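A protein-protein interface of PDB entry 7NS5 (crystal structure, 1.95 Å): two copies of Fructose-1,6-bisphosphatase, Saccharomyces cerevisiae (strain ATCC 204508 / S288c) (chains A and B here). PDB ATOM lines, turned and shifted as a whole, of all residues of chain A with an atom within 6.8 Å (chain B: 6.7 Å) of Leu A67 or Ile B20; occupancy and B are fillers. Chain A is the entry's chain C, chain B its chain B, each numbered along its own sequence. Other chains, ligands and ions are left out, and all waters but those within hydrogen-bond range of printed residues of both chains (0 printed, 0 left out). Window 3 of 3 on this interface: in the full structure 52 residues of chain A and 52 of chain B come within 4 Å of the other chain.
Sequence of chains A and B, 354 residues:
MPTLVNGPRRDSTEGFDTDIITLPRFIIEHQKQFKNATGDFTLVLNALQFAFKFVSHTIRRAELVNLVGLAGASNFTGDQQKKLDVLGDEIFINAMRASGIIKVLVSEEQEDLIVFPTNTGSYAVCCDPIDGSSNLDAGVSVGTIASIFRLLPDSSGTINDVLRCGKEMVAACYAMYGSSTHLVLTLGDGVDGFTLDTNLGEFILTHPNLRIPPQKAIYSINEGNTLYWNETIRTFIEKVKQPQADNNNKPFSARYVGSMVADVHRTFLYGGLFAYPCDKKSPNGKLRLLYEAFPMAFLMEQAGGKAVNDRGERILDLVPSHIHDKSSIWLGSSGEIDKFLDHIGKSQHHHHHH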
ATOM      1  N   ALA A  62      13.226  -1.362  19.294  1.00  0.00           N
ATOM      2  CA  ALA A  62      12.837  -0.543  20.467  1.00  0.00           C
ATOM      3  C   ALA A  62      12.608   0.893  19.987  1.00  0.00           C
ATOM      4  O   ALA A  62      11.925   1.095  18.972  1.00  0.00           O
ATOM      5  CB  ALA A  62      13.879  -0.716  21.575  1.00  0.00           C
ATOM      6  N   GLU A  63      13.198   1.912  20.619  1.00  0.00           N
ATOM      7  CA  GLU A  63      12.888   3.293  20.233  1.00  0.00           C
ATOM      8  C   GLU A  63      13.329   3.615  18.808  1.00  0.00           C
ATOM      9  O   GLU A  63      12.878   4.620  18.238  1.00  0.00           O
ATOM     10  CB  GLU A  63      13.561   4.296  21.180  1.00  0.00           C
ATOM     11  CG  GLU A  63      13.146   4.217  22.628  1.00  0.00           C
ATOM     12  CD  GLU A  63      13.809   3.037  23.333  1.00  0.00           C
ATOM     13  OE1 GLU A  63      13.237   2.544  24.338  1.00  0.00           O
ATOM     14  OE2 GLU A  63      14.891   2.602  22.866  1.00  0.00           O
ATOM     15  N   LEU A  64      14.196   2.793  18.220  1.00  0.00           N
ATOM     16  CA  LEU A  64      14.711   3.137  16.908  1.00  0.00           C
ATOM     17  C   LEU A  64      13.649   3.051  15.821  1.00  0.00           C
ATOM     18  O   LEU A  64      13.880   3.571  14.723  1.00  0.00           O
ATOM     19  CB  LEU A  64      15.911   2.246  16.565  1.00  0.00           C
ATOM     20  CG  LEU A  64      17.055   2.352  17.588  1.00  0.00           C
ATOM     21  CD1 LEU A  64      18.135   1.351  17.231  1.00  0.00           C
ATOM     22  CD2 LEU A  64      17.640   3.785  17.689  1.00  0.00           C
ATOM     23  N   VAL A  65      12.490   2.443  16.105  1.00  0.00           N
ATOM     24  CA  VAL A  65      11.410   2.401  15.117  1.00  0.00           C
ATOM     25  C   VAL A  65      10.936   3.812  14.772  1.00  0.00           C
ATOM     26  O   VAL A  65      10.636   4.119  13.615  1.00  0.00           O
ATOM     27  CB  VAL A  65      10.245   1.529  15.634  1.00  0.00           C
ATOM     28  CG1 VAL A  65      10.655   0.067  15.661  1.00  0.00           C
ATOM     29  CG2 VAL A  65       9.786   2.001  17.024  1.00  0.00           C
ATOM     30  N   ASN A  66      10.859   4.696  15.763  1.00  0.00           N
ATOM     31  CA  ASN A  66      10.396   6.051  15.506  1.00  0.00           C
ATOM     32  C   ASN A  66      11.520   7.052  15.281  1.00  0.00           C
ATOM     33  O   ASN A  66      11.271   8.116  14.715  1.00  0.00           O
ATOM     34  CB  ASN A  66       9.500   6.517  16.657  1.00  0.00           C
ATOM     35  CG  ASN A  66       8.303   5.609  16.845  1.00  0.00           C
ATOM     36  OD1 ASN A  66       7.912   5.295  17.969  1.00  0.00           O
ATOM     37  ND2 ASN A  66       7.692   5.208  15.732  1.00  0.00           N
ATOM     38  N   LEU A  67      12.743   6.731  15.685  1.00  0.00           N
ATOM     39  CA  LEU A  67      13.864   7.650  15.549  1.00  0.00           C
ATOM     40  C   LEU A  67      14.574   7.531  14.208  1.00  0.00           C
ATOM     41  O   LEU A  67      14.932   8.546  13.607  1.00  0.00           O
ATOM     42  CB  LEU A  67      14.862   7.403  16.686  1.00  0.00           C
ATOM     43  CG  LEU A  67      15.986   8.377  17.012  1.00  0.00           C
ATOM     44  CD1 LEU A  67      15.457   9.787  17.167  1.00  0.00           C
ATOM     45  CD2 LEU A  67      16.663   7.928  18.300  1.00  0.00           C
ATOM     46  N   VAL A  68      14.813   6.315  13.728  1.00  0.00           N
ATOM     47  CA  VAL A  68      15.698   6.088  12.589  1.00  0.00           C
ATOM     48  C   VAL A  68      14.847   5.814  11.353  1.00  0.00           C
ATOM     49  O   VAL A  68      14.096   4.831  11.303  1.00  0.00           O
ATOM     50  CB  VAL A  68      16.689   4.944  12.867  1.00  0.00           C
ATOM     51  CG1 VAL A  68      17.626   4.741  11.675  1.00  0.00           C
ATOM     52  CG2 VAL A  68      17.499   5.272  14.099  1.00  0.00           C
ATOM     53  N   GLY A  69      14.948   6.701  10.367  1.00  0.00           N
ATOM     54  CA  GLY A  69      14.253   6.543   9.111  1.00  0.00           C
ATOM     55  C   GLY A  69      15.073   5.736   8.126  1.00  0.00           C
ATOM     56  O   GLY A  69      16.113   5.163   8.451  1.00  0.00           O
ATOM     57  N   ALA A  71      16.954   6.834   5.995  1.00  0.00           N
ATOM     58  CA  ALA A  71      18.188   7.540   5.587  1.00  0.00           C
ATOM     59  C   ALA A  71      18.953   8.237   6.733  1.00  0.00           C
ATOM     60  O   ALA A  71      18.671   8.012   7.921  1.00  0.00           O
ATOM     61  CB  ALA A  71      17.852   8.557   4.498  1.00  0.00           C
ATOM     62  N   GLN A  81       4.166   8.141  13.678  1.00  0.00           N
ATOM     63  CA  GLN A  81       5.004   7.493  14.686  1.00  0.00           C
ATOM     64  C   GLN A  81       4.188   6.524  15.557  1.00  0.00           C
ATOM     65  O   GLN A  81       3.493   6.941  16.485  1.00  0.00           O
ATOM     66  CB  GLN A  81       5.697   8.547  15.558  1.00  0.00           C
ATOM     67  CG  GLN A  81       6.904   9.211  14.890  1.00  0.00           C
ATOM     68  CD  GLN A  81       7.783   9.977  15.873  1.00  0.00           C
ATOM     69  OE1 GLN A  81       7.628   9.859  17.094  1.00  0.00           O
ATOM     70  NE2 GLN A  81       8.726  10.754  15.341  1.00  0.00           N
ATOM     71  N   ILE B  20      20.613  12.287  14.132  1.00  0.00           N
ATOM     72  CA  ILE B  20      21.049  10.973  14.696  1.00  0.00           C
ATOM     73  C   ILE B  20      22.430  11.089  15.343  1.00  0.00           C
ATOM     74  O   ILE B  20      23.394  11.426  14.647  1.00  0.00           O
ATOM     75  CB  ILE B  20      20.898   9.787  13.723  1.00  0.00           C
ATOM     76  CG1 ILE B  20      19.430   9.529  13.377  1.00  0.00           C
ATOM     77  CG2 ILE B  20      21.566   8.538  14.274  1.00  0.00           C
ATOM     78  CD1 ILE B  20      18.532   9.382  14.583  1.00  0.00           C
ATOM     79  N   ILE B  21      22.499  10.813  16.628  1.00  0.00           N
ATOM     80  CA  ILE B  21      23.701  10.875  17.474  1.00  0.00           C
ATOM     81  C   ILE B  21      24.119   9.471  17.900  1.00  0.00           C
ATOM     82  O   ILE B  21      23.401   8.785  18.645  1.00  0.00           O
ATOM     83  CB  ILE B  21      23.500  11.758  18.709  1.00  0.00           C
ATOM     84  CG1 ILE B  21      23.127  13.185  18.298  1.00  0.00           C
ATOM     85  CG2 ILE B  21      24.802  11.806  19.511  1.00  0.00           C
ATOM     86  CD1 ILE B  21      22.761  14.048  19.479  1.00  0.00           C
ATOM     87  N   THR B  22      25.308   9.066  17.485  1.00  0.00           N
ATOM     88  CA  THR B  22      25.858   7.774  17.874  1.00  0.00           C
ATOM     89  C   THR B  22      26.808   7.957  19.052  1.00  0.00           C
ATOM     90  O   THR B  22      27.325   9.049  19.308  1.00  0.00           O
ATOM     91  CB  THR B  22      26.586   7.107  16.705  1.00  0.00           C
ATOM     92  OG1 THR B  22      27.682   7.931  16.294  1.00  0.00           O
ATOM     93  CG2 THR B  22      25.654   6.910  15.502  1.00  0.00           C
ATOM     94  N   ARG B  25      30.374   9.611  18.353  1.00  0.00           N
ATOM     95  CA  ARG B  25      30.347  11.064  18.223  1.00  0.00           C
ATOM     96  C   ARG B  25      29.984  11.757  19.539  1.00  0.00           C
ATOM     97  O   ARG B  25      30.554  12.803  19.870  1.00  0.00           O
ATOM     98  CB  ARG B  25      29.400  11.474  17.093  1.00  0.00           C
ATOM     99  CG  ARG B  25      29.390  12.979  16.865  1.00  0.00           C
ATOM    100  CD  ARG B  25      28.778  13.426  15.524  1.00  0.00           C
ATOM    101  NE  ARG B  25      27.363  13.117  15.325  1.00  0.00           N
ATOM    102  CZ  ARG B  25      26.368  13.895  15.753  1.00  0.00           C
ATOM    103  NH1 ARG B  25      26.637  15.006  16.426  1.00  0.00           N
ATOM    104  NH2 ARG B  25      25.111  13.565  15.513  1.00  0.00           N
ATOM    105  N   LEU B 200      23.091  -1.701  12.191  1.00  0.00           N
ATOM    106  CA  LEU B 200      24.284  -0.893  12.019  1.00  0.00           C
ATOM    107  C   LEU B 200      25.372  -1.196  13.016  1.00  0.00           C
ATOM    108  O   LEU B 200      26.494  -0.719  12.831  1.00  0.00           O
ATOM    109  CB  LEU B 200      23.949   0.594  12.159  1.00  0.00           C
ATOM    110  CG  LEU B 200      22.786   1.135  11.349  1.00  0.00           C
ATOM    111  CD1 LEU B 200      22.581   2.589  11.717  1.00  0.00           C
ATOM    112  CD2 LEU B 200      23.169   0.972   9.879  1.00  0.00           C
ATOM    113  N   ILE B 204      22.881   4.273  19.618  1.00  0.00           N
ATOM    114  CA  ILE B 204      22.276   5.534  19.210  1.00  0.00           C
ATOM    115  C   ILE B 204      21.583   6.153  20.408  1.00  0.00           C
ATOM    116  O   ILE B 204      20.879   5.455  21.158  1.00  0.00           O
ATOM    117  CB  ILE B 204      21.326   5.322  18.019  1.00  0.00           C
ATOM    118  CG1 ILE B 204      22.186   4.979  16.780  1.00  0.00           C
ATOM    119  CG2 ILE B 204      20.465   6.550  17.784  1.00  0.00           C
ATOM    120  CD1 ILE B 204      21.405   4.647  15.537  1.00  0.00           C
ATOM    121  N   LEU B 205      21.799   7.456  20.587  1.00  0.00           N
ATOM    122  CA  LEU B 205      21.233   8.212  21.695  1.00  0.00           C
ATOM    123  C   LEU B 205      19.704   8.244  21.616  1.00  0.00           C
ATOM    124  O   LEU B 205      19.123   8.745  20.648  1.00  0.00           O
ATOM    125  CB  LEU B 205      21.811   9.627  21.694  1.00  0.00           C
ATOM    126  CG  LEU B 205      21.391  10.546  22.851  1.00  0.00           C
ATOM    127  CD1 LEU B 205      21.748   9.948  24.212  1.00  0.00           C
ATOM    128  CD2 LEU B 205      22.010  11.931  22.712  1.00  0.00           C
ATOM    129  N   THR B 206      19.054   7.662  22.624  1.00  0.00           N
ATOM    130  CA  THR B 206      17.605   7.618  22.654  1.00  0.00           C
ATOM    131  C   THR B 206      17.018   8.177  23.928  1.00  0.00           C
ATOM    132  O   THR B 206      15.828   8.489  23.936  1.00  0.00           O
ATOM    133  CB  THR B 206      17.093   6.186  22.456  1.00  0.00           C
ATOM    134  OG1 THR B 206      17.783   5.293  23.340  1.00  0.00           O
ATOM    135  CG2 THR B 206      17.336   5.730  21.028  1.00  0.00           C
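Among the printed residues, merely in contact across the chains: Glu A63 with Thr B206, Leu A64 with Ile B204, Leu A64 with Thr B206, Leu A67 with Ile B20, Leu A67 with Leu B205 and Leu A67 with Thr B206.
Printed residues of chain B within 4 Å of Glu A63: Thr B206.
Of the printed residues of chain B, Leu A64 touches Ile B204 (3.95 Å) and Thr B206 (3.9 Å).
Leu A67 touches just these residues of chain B: Ile B20, Leu B205 and Thr B206.
Of chain A, only Leu A67 comes within 4 Å of Ile B20.
Printed residues of chain A within 4 Å of Ile B204: Leu A64.
Of the printed residues of chain A, Leu B205 touches Leu A67 (3.5 Å).
Of the printed residues of chain A, Thr B206 touches Glu A63 (3.98 Å), Leu A64 (3.9 Å) and Leu A67 (3.6 Å).
The nearest residue of chain B that does not touch Leu A67 is Ile B204 (4.1 Å).
The nearest printed residue of chain A that does not touch Leu B205 is Leu A64 (6.0 Å).
The backbone carbonyl oxygen of Ile B20 sits at hydrogen-bond distance from the guanidinium group of Arg B25 (2.9 Å).
The backbone carbonyl oxygen of Ile B21 sits at hydrogen-bond distance from the backbone NH of Leu B205.
Printed residues of chain A that touch a printed residue of chain B: Glu A63, Leu A64 and Leu A67.
Hydrophobic or aromatic side chains of chain A that line the printed part of chain B: Leu A64 and Leu A67.
Of the 8 printed residues of chain B, 4 touch a printed residue of chain A.
Among the printed residues, 6 pairs touch across the chains.
No position is printed for both chains.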
